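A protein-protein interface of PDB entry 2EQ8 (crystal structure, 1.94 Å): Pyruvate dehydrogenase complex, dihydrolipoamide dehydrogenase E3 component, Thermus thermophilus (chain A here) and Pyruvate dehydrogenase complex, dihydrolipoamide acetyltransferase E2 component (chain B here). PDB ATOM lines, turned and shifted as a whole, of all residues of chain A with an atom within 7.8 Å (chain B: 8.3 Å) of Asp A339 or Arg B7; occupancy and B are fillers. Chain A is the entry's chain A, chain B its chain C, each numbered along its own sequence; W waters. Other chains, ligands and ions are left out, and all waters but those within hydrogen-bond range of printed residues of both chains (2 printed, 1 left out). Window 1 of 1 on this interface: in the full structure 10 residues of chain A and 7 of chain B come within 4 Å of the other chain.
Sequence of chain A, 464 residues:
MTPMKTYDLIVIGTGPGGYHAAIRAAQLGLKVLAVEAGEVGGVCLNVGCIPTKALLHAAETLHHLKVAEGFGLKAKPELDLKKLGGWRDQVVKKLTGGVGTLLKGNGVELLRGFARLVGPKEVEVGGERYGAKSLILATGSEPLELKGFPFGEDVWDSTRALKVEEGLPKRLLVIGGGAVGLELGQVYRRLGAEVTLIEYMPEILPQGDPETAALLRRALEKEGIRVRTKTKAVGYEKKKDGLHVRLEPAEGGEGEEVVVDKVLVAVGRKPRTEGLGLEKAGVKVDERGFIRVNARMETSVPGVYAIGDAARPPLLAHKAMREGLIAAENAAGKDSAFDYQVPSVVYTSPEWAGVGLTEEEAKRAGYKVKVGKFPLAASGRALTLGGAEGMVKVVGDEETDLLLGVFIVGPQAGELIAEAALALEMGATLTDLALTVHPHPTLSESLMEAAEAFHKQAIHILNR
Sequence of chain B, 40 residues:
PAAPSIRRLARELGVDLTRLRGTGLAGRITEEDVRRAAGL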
ATOM      1  N   ALA A 295       9.462  18.507 -20.515  1.00  0.00           N
ATOM      2  CA  ALA A 295      10.770  19.148 -20.380  1.00  0.00           C
ATOM      3  C   ALA A 295      11.896  18.387 -21.066  1.00  0.00           C
ATOM      4  O   ALA A 295      12.929  18.966 -21.414  1.00  0.00           O
ATOM      5  CB  ALA A 295      11.101  19.343 -18.900  1.00  0.00           C
ATOM      6  N   MET A 297      11.517  17.051 -23.851  1.00  0.00           N
ATOM      7  CA  MET A 297      11.173  17.170 -25.266  1.00  0.00           C
ATOM      8  C   MET A 297      10.507  15.888 -25.774  1.00  0.00           C
ATOM      9  O   MET A 297      10.372  15.681 -26.982  1.00  0.00           O
ATOM     10  CB  MET A 297      12.420  17.475 -26.112  1.00  0.00           C
ATOM     11  CG  MET A 297      13.243  18.673 -25.628  1.00  0.00           C
ATOM     12  SD  MET A 297      12.240  20.133 -25.223  1.00  0.00           S
ATOM     13  CE  MET A 297      11.477  20.456 -26.806  1.00  0.00           C
ATOM     14  N   ARG A 312       6.636  23.962 -29.814  1.00  0.00           N
ATOM     15  CA  ARG A 312       6.022  25.014 -29.013  1.00  0.00           C
ATOM     16  C   ARG A 312       6.682  26.372 -29.216  1.00  0.00           C
ATOM     17  O   ARG A 312       7.837  26.460 -29.638  1.00  0.00           O
ATOM     18  CB  ARG A 312       6.155  24.647 -27.532  1.00  0.00           C
ATOM     19  CG  ARG A 312       7.623  24.511 -27.118  1.00  0.00           C
ATOM     20  CD  ARG A 312       7.821  23.861 -25.756  1.00  0.00           C
ATOM     21  NE  ARG A 312       9.244  23.779 -25.425  1.00  0.00           N
ATOM     22  CZ  ARG A 312       9.729  23.287 -24.288  1.00  0.00           C
ATOM     23  NH1 ARG A 312       8.909  22.820 -23.354  1.00  0.00           N
ATOM     24  NH2 ARG A 312      11.039  23.279 -24.079  1.00  0.00           N
ATOM     25  N   ARG A 322      18.812  24.464 -28.893  1.00  0.00           N
ATOM     26  CA  ARG A 322      18.979  23.869 -27.566  1.00  0.00           C
ATOM     27  C   ARG A 322      18.050  22.666 -27.395  1.00  0.00           C
ATOM     28  O   ARG A 322      18.452  21.628 -26.866  1.00  0.00           O
ATOM     29  CB  ARG A 322      18.687  24.902 -26.471  1.00  0.00           C
ATOM     30  CG  ARG A 322      18.786  24.347 -25.046  1.00  0.00           C
ATOM     31  CD  ARG A 322      20.135  23.693 -24.813  1.00  0.00           C
ATOM     32  NE  ARG A 322      21.227  24.636 -25.028  1.00  0.00           N
ATOM     33  CZ  ARG A 322      21.669  25.495 -24.115  1.00  0.00           C
ATOM     34  NH1 ARG A 322      21.122  25.529 -22.905  1.00  0.00           N
ATOM     35  NH2 ARG A 322      22.643  26.340 -24.424  1.00  0.00           N
ATOM     36  N   ILE A 326      18.931  18.736 -26.351  1.00  0.00           N
ATOM     37  CA  ILE A 326      18.280  18.000 -25.265  1.00  0.00           C
ATOM     38  C   ILE A 326      17.681  16.684 -25.779  1.00  0.00           C
ATOM     39  O   ILE A 326      17.853  15.625 -25.169  1.00  0.00           O
ATOM     40  CB  ILE A 326      17.144  18.836 -24.626  1.00  0.00           C
ATOM     41  CG1 ILE A 326      17.687  20.180 -24.122  1.00  0.00           C
ATOM     42  CG2 ILE A 326      16.499  18.049 -23.486  1.00  0.00           C
ATOM     43  CD1 ILE A 326      18.769  20.071 -23.061  1.00  0.00           C
ATOM     44  N   ASP A 335      19.847  12.160 -19.472  1.00  0.00           N
ATOM     45  CA  ASP A 335      18.642  12.708 -18.871  1.00  0.00           C
ATOM     46  C   ASP A 335      18.754  14.224 -18.830  1.00  0.00           C
ATOM     47  O   ASP A 335      19.134  14.806 -17.812  1.00  0.00           O
ATOM     48  CB  ASP A 335      18.442  12.172 -17.451  1.00  0.00           C
ATOM     49  CG  ASP A 335      17.065  12.504 -16.895  1.00  0.00           C
ATOM     50  OD1 ASP A 335      16.461  13.500 -17.349  1.00  0.00           O
ATOM     51  OD2 ASP A 335      16.588  11.778 -15.999  1.00  0.00           O
ATOM     52  N   SER A 336      18.430  14.862 -19.951  1.00  0.00           N
ATOM     53  CA  SER A 336      18.491  16.314 -20.044  1.00  0.00           C
ATOM     54  C   SER A 336      17.090  16.905 -20.078  1.00  0.00           C
ATOM     55  O   SER A 336      16.139  16.251 -20.510  1.00  0.00           O
ATOM     56  CB  SER A 336      19.254  16.734 -21.307  1.00  0.00           C
ATOM     57  OG  SER A 336      20.601  16.299 -21.252  1.00  0.00           O
ATOM     58  N   ALA A 337      16.966  18.143 -19.615  1.00  0.00           N
ATOM     59  CA  ALA A 337      15.678  18.817 -19.607  1.00  0.00           C
ATOM     60  C   ALA A 337      15.854  20.274 -20.010  1.00  0.00           C
ATOM     61  O   ALA A 337      16.904  20.870 -19.779  1.00  0.00           O
ATOM     62  CB  ALA A 337      15.045  18.726 -18.222  1.00  0.00           C
ATOM     63  N   PHE A 338      14.830  20.850 -20.623  1.00  0.00           N
ATOM     64  CA  PHE A 338      14.915  22.245 -21.026  1.00  0.00           C
ATOM     65  C   PHE A 338      14.302  23.079 -19.909  1.00  0.00           C
ATOM     66  O   PHE A 338      13.102  23.006 -19.654  1.00  0.00           O
ATOM     67  CB  PHE A 338      14.171  22.461 -22.345  1.00  0.00           C
ATOM     68  CG  PHE A 338      14.403  23.814 -22.962  1.00  0.00           C
ATOM     69  CD1 PHE A 338      13.847  24.961 -22.395  1.00  0.00           C
ATOM     70  CD2 PHE A 338      15.163  23.938 -24.120  1.00  0.00           C
ATOM     71  CE1 PHE A 338      14.042  26.213 -22.972  1.00  0.00           C
ATOM     72  CE2 PHE A 338      15.367  25.188 -24.712  1.00  0.00           C
ATOM     73  CZ  PHE A 338      14.803  26.329 -24.136  1.00  0.00           C
ATOM     74  N   ASP A 339      15.142  23.847 -19.224  1.00  0.00           N
ATOM     75  CA  ASP A 339      14.705  24.701 -18.125  1.00  0.00           C
ATOM     76  C   ASP A 339      15.486  26.008 -18.204  1.00  0.00           C
ATOM     77  O   ASP A 339      15.812  26.615 -17.185  1.00  0.00           O
ATOM     78  CB  ASP A 339      14.996  24.011 -16.788  1.00  0.00           C
ATOM     79  CG  ASP A 339      16.482  23.772 -16.561  1.00  0.00           C
ATOM     80  OD1 ASP A 339      17.293  24.138 -17.439  1.00  0.00           O
ATOM     81  OD2 ASP A 339      16.848  23.220 -15.500  1.00  0.00           O
ATOM     82  N   TYR A 340      15.772  26.443 -19.427  1.00  0.00           N
ATOM     83  CA  TYR A 340      16.561  27.646 -19.640  1.00  0.00           C
ATOM     84  C   TYR A 340      15.791  28.919 -19.960  1.00  0.00           C
ATOM     85  O   TYR A 340      14.632  28.878 -20.358  1.00  0.00           O
ATOM     86  CB  TYR A 340      17.574  27.377 -20.755  1.00  0.00           C
ATOM     87  CG  TYR A 340      18.350  26.101 -20.536  1.00  0.00           C
ATOM     88  CD1 TYR A 340      17.905  24.887 -21.064  1.00  0.00           C
ATOM     89  CD2 TYR A 340      19.489  26.093 -19.737  1.00  0.00           C
ATOM     90  CE1 TYR A 340      18.578  23.698 -20.793  1.00  0.00           C
ATOM     91  CE2 TYR A 340      20.163  24.917 -19.462  1.00  0.00           C
ATOM     92  CZ  TYR A 340      19.708  23.727 -19.986  1.00  0.00           C
ATOM     93  OH  TYR A 340      20.382  22.567 -19.687  1.00  0.00           O
ATOM     94  N   GLN A 341      16.460  30.052 -19.759  1.00  0.00           N
ATOM     95  CA  GLN A 341      15.890  31.360 -20.056  1.00  0.00           C
ATOM     96  C   GLN A 341      16.089  31.560 -21.550  1.00  0.00           C
ATOM     97  O   GLN A 341      17.189  31.361 -22.064  1.00  0.00           O
ATOM     98  CB  GLN A 341      16.633  32.460 -19.297  1.00  0.00           C
ATOM     99  CG  GLN A 341      16.437  32.448 -17.793  1.00  0.00           C
ATOM    100  CD  GLN A 341      15.007  32.747 -17.400  1.00  0.00           C
ATOM    101  OE1 GLN A 341      14.401  33.691 -17.904  1.00  0.00           O
ATOM    102  NE2 GLN A 341      14.460  31.948 -16.494  1.00  0.00           N
ATOM    103  N   VAL A 342      15.031  31.946 -22.247  1.00  0.00           N
ATOM    104  CA  VAL A 342      15.115  32.151 -23.686  1.00  0.00           C
ATOM    105  C   VAL A 342      15.001  33.627 -24.025  1.00  0.00           C
ATOM    106  O   VAL A 342      13.955  34.231 -23.826  1.00  0.00           O
ATOM    107  CB  VAL A 342      13.981  31.399 -24.422  1.00  0.00           C
ATOM    108  CG1 VAL A 342      14.128  31.578 -25.932  1.00  0.00           C
ATOM    109  CG2 VAL A 342      14.007  29.919 -24.041  1.00  0.00           C
ATOM    110  N   LEU A 424      20.694  35.638 -15.309  1.00  0.00           N
ATOM    111  CA  LEU A 424      19.523  34.908 -14.825  1.00  0.00           C
ATOM    112  C   LEU A 424      19.842  33.436 -14.561  1.00  0.00           C
ATOM    113  O   LEU A 424      19.447  32.886 -13.533  1.00  0.00           O
ATOM    114  CB  LEU A 424      18.368  35.015 -15.823  1.00  0.00           C
ATOM    115  CG  LEU A 424      17.760  36.408 -16.011  1.00  0.00           C
ATOM    116  CD1 LEU A 424      16.762  36.369 -17.158  1.00  0.00           C
ATOM    117  CD2 LEU A 424      17.084  36.865 -14.718  1.00  0.00           C
ATOM    118  N   GLU A 425      20.562  32.798 -15.482  1.00  0.00           N
ATOM    119  CA  GLU A 425      20.915  31.394 -15.313  1.00  0.00           C
ATOM    120  C   GLU A 425      21.725  31.169 -14.041  1.00  0.00           C
ATOM    121  O   GLU A 425      21.584  30.136 -13.386  1.00  0.00           O
ATOM    122  CB  GLU A 425      21.706  30.887 -16.520  1.00  0.00           C
ATOM    123  CG  GLU A 425      20.903  30.809 -17.807  1.00  0.00           C
ATOM    124  CD  GLU A 425      19.786  29.774 -17.750  1.00  0.00           C
ATOM    125  OE1 GLU A 425      19.030  29.660 -18.739  1.00  0.00           O
ATOM    126  OE2 GLU A 425      19.667  29.075 -16.721  1.00  0.00           O
ATOM    127  N   MET A 426      22.570  32.139 -13.695  1.00  0.00           N
ATOM    128  CA  MET A 426      23.407  32.042 -12.503  1.00  0.00           C
ATOM    129  C   MET A 426      22.709  32.566 -11.252  1.00  0.00           C
ATOM    130  O   MET A 426      23.319  32.632 -10.188  1.00  0.00           O
ATOM    131  CB  MET A 426      24.711  32.822 -12.700  1.00  0.00           C
ATOM    132  CG  MET A 426      25.575  32.350 -13.859  1.00  0.00           C
ATOM    133  SD  MET A 426      26.061  30.620 -13.722  1.00  0.00           S
ATOM    134  CE  MET A 426      27.089  30.670 -12.271  1.00  0.00           C
ATOM    135  N   GLY A 427      21.443  32.945 -11.377  1.00  0.00           N
ATOM    136  CA  GLY A 427      20.712  33.457 -10.227  1.00  0.00           C
ATOM    137  C   GLY A 427      21.324  34.723  -9.650  1.00  0.00           C
ATOM    138  O   GLY A 427      21.400  34.897  -8.434  1.00  0.00           O
ATOM    139  N   PRO B   1      17.890  30.954  -8.248  1.00  0.00           N
ATOM    140  CA  PRO B   1      17.948  29.553  -8.731  1.00  0.00           C
ATOM    141  C   PRO B   1      19.382  29.047  -8.845  1.00  0.00           C
ATOM    142  O   PRO B   1      20.332  29.798  -8.614  1.00  0.00           O
ATOM    143  CB  PRO B   1      17.238  29.513 -10.078  1.00  0.00           C
ATOM    144  CG  PRO B   1      17.312  30.979 -10.512  1.00  0.00           C
ATOM    145  CD  PRO B   1      17.173  31.792  -9.225  1.00  0.00           C
ATOM    146  N   ALA B   2      19.538  27.773  -9.194  1.00  0.00           N
ATOM    147  CA  ALA B   2      20.863  27.176  -9.316  1.00  0.00           C
ATOM    148  C   ALA B   2      21.410  27.291 -10.731  1.00  0.00           C
ATOM    149  O   ALA B   2      20.656  27.327 -11.702  1.00  0.00           O
ATOM    150  CB  ALA B   2      20.821  25.708  -8.890  1.00  0.00           C
ATOM    151  N   ALA B   3      22.732  27.359 -10.833  1.00  0.00           N
ATOM    152  CA  ALA B   3      23.405  27.471 -12.120  1.00  0.00           C
ATOM    153  C   ALA B   3      23.124  26.249 -12.996  1.00  0.00           C
ATOM    154  O   ALA B   3      22.924  25.146 -12.493  1.00  0.00           O
ATOM    155  CB  ALA B   3      24.897  27.634 -11.902  1.00  0.00           C
ATOM    156  N   PRO B   4      23.112  26.433 -14.327  1.00  0.00           N
ATOM    157  CA  PRO B   4      22.855  25.350 -15.280  1.00  0.00           C
ATOM    158  C   PRO B   4      23.619  24.056 -14.994  1.00  0.00           C
ATOM    159  O   PRO B   4      23.049  22.972 -15.046  1.00  0.00           O
ATOM    160  CB  PRO B   4      23.256  25.969 -16.615  1.00  0.00           C
ATOM    161  CG  PRO B   4      22.867  27.404 -16.433  1.00  0.00           C
ATOM    162  CD  PRO B   4      23.380  27.698 -15.035  1.00  0.00           C
ATOM    163  N   SER B   5      24.904  24.185 -14.689  1.00  0.00           N
ATOM    164  CA  SER B   5      25.761  23.035 -14.417  1.00  0.00           C
ATOM    165  C   SER B   5      25.314  22.237 -13.196  1.00  0.00           C
ATOM    166  O   SER B   5      25.431  21.007 -13.159  1.00  0.00           O
ATOM    167  CB  SER B   5      27.198  23.504 -14.206  1.00  0.00           C
ATOM    168  OG  SER B   5      28.056  22.394 -14.044  1.00  0.00           O
ATOM    169  N   ILE B   6      24.825  22.948 -12.190  1.00  0.00           N
ATOM    170  CA  ILE B   6      24.349  22.313 -10.966  1.00  0.00           C
ATOM    171  C   ILE B   6      23.004  21.636 -11.214  1.00  0.00           C
ATOM    172  O   ILE B   6      22.751  20.533 -10.727  1.00  0.00           O
ATOM    173  CB  ILE B   6      24.218  23.355  -9.840  1.00  0.00           C
ATOM    174  CG1 ILE B   6      25.618  23.804  -9.414  1.00  0.00           C
ATOM    175  CG2 ILE B   6      23.439  22.774  -8.660  1.00  0.00           C
ATOM    176  CD1 ILE B   6      25.629  24.999  -8.498  1.00  0.00           C
ATOM    177  N   ARG B   7      22.145  22.297 -11.982  1.00  0.00           N
ATOM    178  CA  ARG B   7      20.843  21.729 -12.292  1.00  0.00           C
ATOM    179  C   ARG B   7      21.043  20.456 -13.110  1.00  0.00           C
ATOM    180  O   ARG B   7      20.369  19.447 -12.889  1.00  0.00           O
ATOM    181  CB  ARG B   7      19.991  22.731 -13.082  1.00  0.00           C
ATOM    182  CG  ARG B   7      19.869  24.090 -12.408  1.00  0.00           C
ATOM    183  CD  ARG B   7      18.687  24.883 -12.936  1.00  0.00           C
ATOM    184  NE  ARG B   7      18.698  25.071 -14.387  1.00  0.00           N
ATOM    185  CZ  ARG B   7      19.220  26.122 -15.014  1.00  0.00           C
ATOM    186  NH1 ARG B   7      19.793  27.105 -14.328  1.00  0.00           N
ATOM    187  NH2 ARG B   7      19.134  26.207 -16.336  1.00  0.00           N
ATOM    188  N   ARG B   8      21.979  20.507 -14.055  1.00  0.00           N
ATOM    189  CA  ARG B   8      22.258  19.357 -14.906  1.00  0.00           C
ATOM    190  C   ARG B   8      22.871  18.216 -14.094  1.00  0.00           C
ATOM    191  O   ARG B   8      22.484  17.060 -14.251  1.00  0.00           O
ATOM    192  CB  ARG B   8      23.193  19.769 -16.057  1.00  0.00           C
ATOM    193  CG  ARG B   8      23.491  18.673 -17.091  1.00  0.00           C
ATOM    194  CD  ARG B   8      22.226  18.058 -17.687  1.00  0.00           C
ATOM    195  NE  ARG B   8      21.447  18.964 -18.537  1.00  0.00           N
ATOM    196  CZ  ARG B   8      21.801  19.355 -19.761  1.00  0.00           C
ATOM    197  NH1 ARG B   8      21.013  20.176 -20.450  1.00  0.00           N
ATOM    198  NH2 ARG B   8      22.939  18.930 -20.304  1.00  0.00           N
ATOM    199  N   LEU B   9      23.815  18.543 -13.217  1.00  0.00           N
ATOM    200  CA  LEU B   9      24.465  17.535 -12.382  1.00  0.00           C
ATOM    201  C   LEU B   9      23.428  16.847 -11.487  1.00  0.00           C
ATOM    202  O   LEU B   9      23.491  15.641 -11.259  1.00  0.00           O
ATOM    203  CB  LEU B   9      25.535  18.188 -11.499  1.00  0.00           C
ATOM    204  CG  LEU B   9      26.810  17.414 -11.128  1.00  0.00           C
ATOM    205  CD1 LEU B   9      27.278  17.886  -9.762  1.00  0.00           C
ATOM    206  CD2 LEU B   9      26.578  15.921 -11.111  1.00  0.00           C
ATOM    207  N   ALA B  10      22.471  17.618 -10.984  1.00  0.00           N
ATOM    208  CA  ALA B  10      21.434  17.067 -10.113  1.00  0.00           C
ATOM    209  C   ALA B  10      20.595  16.019 -10.853  1.00  0.00           C
ATOM    210  O   ALA B  10      20.242  14.979 -10.291  1.00  0.00           O
ATOM    211  CB  ALA B  10      20.545  18.187  -9.580  1.00  0.00           C
ATOM    212  N   ARG B  11      20.281  16.289 -12.116  1.00  0.00           N
ATOM    213  CA  ARG B  11      19.505  15.344 -12.907  1.00  0.00           C
ATOM    214  C   ARG B  11      20.328  14.080 -13.111  1.00  0.00           C
ATOM    215  O   ARG B  11      19.816  12.963 -13.021  1.00  0.00           O
ATOM    216  CB  ARG B  11      19.162  15.924 -14.279  1.00  0.00           C
ATOM    217  CG  ARG B  11      18.230  17.124 -14.265  1.00  0.00           C
ATOM    218  CD  ARG B  11      17.767  17.435 -15.683  1.00  0.00           C
ATOM    219  NE  ARG B  11      16.813  16.442 -16.179  1.00  0.00           N
ATOM    220  CZ  ARG B  11      15.529  16.397 -15.826  1.00  0.00           C
ATOM    221  NH1 ARG B  11      15.043  17.293 -14.976  1.00  0.00           N
ATOM    222  NH2 ARG B  11      14.727  15.464 -16.328  1.00  0.00           N
ATOM    223  N   GLU B  12      21.607  14.271 -13.400  1.00  0.00           N
ATOM    224  CA  GLU B  12      22.510  13.153 -13.630  1.00  0.00           C
ATOM    225  C   GLU B  12      22.611  12.256 -12.398  1.00  0.00           C
ATOM    226  O   GLU B  12      22.541  11.033 -12.503  1.00  0.00           O
ATOM    227  CB  GLU B  12      23.901  13.677 -13.986  1.00  0.00           C
ATOM    228  CG  GLU B  12      24.884  12.597 -14.397  1.00  0.00           C
ATOM    229  CD  GLU B  12      26.303  13.116 -14.486  1.00  0.00           C
ATOM    230  OE1 GLU B  12      26.507  14.192 -15.092  1.00  0.00           O
ATOM    231  OE2 GLU B  12      27.215  12.446 -13.952  1.00  0.00           O
ATOM    232  N   LEU B  13      22.767  12.870 -11.229  1.00  0.00           N
ATOM    233  CA  LEU B  13      22.905  12.119  -9.984  1.00  0.00           C
ATOM    234  C   LEU B  13      21.592  11.741  -9.308  1.00  0.00           C
ATOM    235  O   LEU B  13      21.603  11.122  -8.247  1.00  0.00           O
ATOM    236  CB  LEU B  13      23.783  12.901  -9.003  1.00  0.00           C
ATOM    237  CG  LEU B  13      25.179  13.273  -9.513  1.00  0.00           C
ATOM    238  CD1 LEU B  13      25.966  13.952  -8.399  1.00  0.00           C
ATOM    239  CD2 LEU B  13      25.907  12.023  -9.996  1.00  0.00           C
ATOM    240  N   GLY B  14      20.469  12.108  -9.921  1.00  0.00           N
ATOM    241  CA  GLY B  14      19.167  11.786  -9.357  1.00  0.00           C
ATOM    242  C   GLY B  14      18.867  12.533  -8.070  1.00  0.00           C
ATOM    243  O   GLY B  14      18.182  12.018  -7.178  1.00  0.00           O
ATOM    244  N   VAL B  15      19.383  13.752  -7.969  1.00  0.00           N
ATOM    245  CA  VAL B  15      19.175  14.574  -6.785  1.00  0.00           C
ATOM    246  C   VAL B  15      18.086  15.598  -7.067  1.00  0.00           C
ATOM    247  O   VAL B  15      18.077  16.220  -8.125  1.00  0.00           O
ATOM    248  CB  VAL B  15      20.475  15.309  -6.380  1.00  0.00           C
ATOM    249  CG1 VAL B  15      20.191  16.316  -5.275  1.00  0.00           C
ATOM    250  CG2 VAL B  15      21.516  14.303  -5.910  1.00  0.00           C
ATOM    251  N   LEU B  17      16.847  19.020  -6.344  1.00  0.00           N
ATOM    252  CA  LEU B  17      17.291  20.281  -5.765  1.00  0.00           C
ATOM    253  C   LEU B  17      16.282  20.948  -4.831  1.00  0.00           C
ATOM    254  O   LEU B  17      16.682  21.619  -3.884  1.00  0.00           O
ATOM    255  CB  LEU B  17      17.687  21.268  -6.869  1.00  0.00           C
ATOM    256  CG  LEU B  17      18.864  20.870  -7.769  1.00  0.00           C
ATOM    257  CD1 LEU B  17      19.139  21.990  -8.765  1.00  0.00           C
ATOM    258  CD2 LEU B  17      20.107  20.601  -6.915  1.00  0.00           C
ATOM    259  N   ILE B  29      23.165  26.705  -3.802  1.00  0.00           N
ATOM    260  CA  ILE B  29      23.470  25.282  -3.861  1.00  0.00           C
ATOM    261  C   ILE B  29      24.788  25.088  -4.605  1.00  0.00           C
ATOM    262  O   ILE B  29      24.944  25.557  -5.732  1.00  0.00           O
ATOM    263  CB  ILE B  29      22.347  24.500  -4.588  1.00  0.00           C
ATOM    264  CG1 ILE B  29      21.048  24.585  -3.779  1.00  0.00           C
ATOM    265  CG2 ILE B  29      22.764  23.046  -4.776  1.00  0.00           C
ATOM    266  CD1 ILE B  29      19.859  23.917  -4.442  1.00  0.00           C
ATOM    267  N   THR B  30      25.735  24.406  -3.966  1.00  0.00           N
ATOM    268  CA  THR B  30      27.044  24.157  -4.568  1.00  0.00           C
ATOM    269  C   THR B  30      27.093  22.775  -5.196  1.00  0.00           C
ATOM    270  O   THR B  30      26.208  21.947  -4.972  1.00  0.00           O
ATOM    271  CB  THR B  30      28.177  24.234  -3.526  1.00  0.00           C
ATOM    272  OG1 THR B  30      28.061  23.138  -2.609  1.00  0.00           O
ATOM    273  CG2 THR B  30      28.106  25.549  -2.757  1.00  0.00           C
ATOM    274  N   GLU B  31      28.130  22.528  -5.987  1.00  0.00           N
ATOM    275  CA  GLU B  31      28.277  21.233  -6.627  1.00  0.00           C
ATOM    276  C   GLU B  31      28.436  20.178  -5.547  1.00  0.00           C
ATOM    277  O   GLU B  31      27.870  19.090  -5.642  1.00  0.00           O
ATOM    278  CB  GLU B  31      29.504  21.211  -7.538  1.00  0.00           C
ATOM    279  CG  GLU B  31      29.690  19.882  -8.252  1.00  0.00           C
ATOM    280  CD  GLU B  31      30.922  19.859  -9.132  1.00  0.00           C
ATOM    281  OE1 GLU B  31      31.134  20.838  -9.877  1.00  0.00           O
ATOM    282  OE2 GLU B  31      31.671  18.860  -9.086  1.00  0.00           O
ATOM    283  N   VAL B  34      25.258  19.010  -4.058  1.00  0.00           N
ATOM    284  CA  VAL B  34      24.580  18.008  -4.868  1.00  0.00           C
ATOM    285  C   VAL B  34      25.218  16.634  -4.686  1.00  0.00           C
ATOM    286  O   VAL B  34      24.523  15.637  -4.481  1.00  0.00           O
ATOM    287  CB  VAL B  34      24.618  18.394  -6.360  1.00  0.00           C
ATOM    288  CG1 VAL B  34      23.898  17.352  -7.188  1.00  0.00           C
ATOM    289  CG2 VAL B  34      23.970  19.764  -6.554  1.00  0.00           C
HETATM  290  O   HOH W   1      20.453  22.806 -16.957  1.00  0.00           O
HETATM  291  O   HOH W   2      21.980  14.799 -16.497  1.00  0.00           O
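The side-chain carboxylate (OD1) of Asp A335 lies within salt-bridge range of the guanidinium group (NH2) of Arg B11 (2.8 Å).
The side-chain carboxylate (OD2) of Asp A339 is in salt-bridge range of the guanidinium group (NE) of Arg B7, at 2.8 Å.
NH1 of Arg B8 is in hydrogen-bond range of OH of Tyr A340 (2.6 Å).
OE2 of Glu A425 lies within salt-bridge range of NH2 of Arg B7 (2.9 Å).
The backbone carbonyl oxygen (O) of Ala B2 lies close to the backbone carbonyl oxygen (O) of Glu A425 (3.4 Å).
The side-chain carboxylate of Glu A425 is in hydrogen-bond range of the backbone NH of Gln A341, at 2.8 Å.
O of Ala B2 is in hydrogen-bond range of NH1 of Arg B7, at 2.8 Å.
Ile A326 touches Arg B8 (CD1 to NH1, 3.4 Å).
Arg B8 touches Ser A336.
NE of Arg B11 touches C of Ser A336, 3.9 Å away.
Ala A337 touches Arg B11.
NH2 of Arg B7 touches CD2 of Tyr A340, 3.4 Å away.
Glu A425 touches Ala B3 (O to CA, 3.5 Å).
Glu A425 touches Pro B4 (O to CD, 3.4 Å).
Met A426 touches Ala B3 (SD to CB, 3.7 Å).
Of chain B, only Arg B7 (2.8 Å) comes within 4 Å of Asp A339.
Of chain A, only Asp A339 (2.8 Å), Tyr A340 (3.4 Å) and Glu A425 (2.9 Å) come within 4 Å of Arg B7.
Of chain B, only Arg B7 (3.4 Å) and Arg B8 (2.6 Å) come within 4 Å of Tyr A340.
Printed residues of chain B within 4 Å of Met A426: Ala B3 (3.7 Å).
Of the printed residues of chain B, Ser A336 touches Arg B8 (3.6 Å) and Arg B11 (3.9 Å).
Of the printed residues of chain A, Arg B8 touches Ile A326 (3.4 Å), Ser A336 (3.6 Å) and Tyr A340 (2.6 Å).
Of the printed residues of chain B, Ile A326 touches Arg B8 (3.4 Å).
Printed residues of chain A within 4 Å of Ala B2: Glu A425.
The nearest residue of chain B that does not touch Asp A339 is Arg B11 (5.9 Å).
The nearest printed residue of chain A that does not touch Arg B7 is Met A426 (5.8 Å).
The nearest printed residue of chain B that does not touch Ala A337 is Arg B8 (4.2 Å).
Of the 20 printed residues of chain B, 6 touch a printed residue of chain A.
Printed residues of chain B that touch a printed residue of chain A: Ala B2, Ala B3, Pro B4, Arg B7, Arg B8 and Arg B11.
Hydrophobic or aromatic side chains of chain A that line the printed part of chain B: Ile A326, Ala A337, Tyr A340 and Met A426.
Among the printed residues, Asp or Glu carboxylates within 4 Å of a Lys or Arg side-chain nitrogen of the other chain: Asp A335 with Arg B11 (2.8 Å), Asp A339 with Arg B7 (2.8 Å) and Glu A425 with Arg B7 (2.9 Å).
Water W1 lies within hydrogen-bond range of OH of Tyr A340, O of Pro B4 and OD1 of Asp A339.
Water W2 lies within hydrogen-bond range of O of Asp A335 (3.1 Å), N of Glu B12 (3.2 Å) and O of Arg B8 (3.2 Å).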
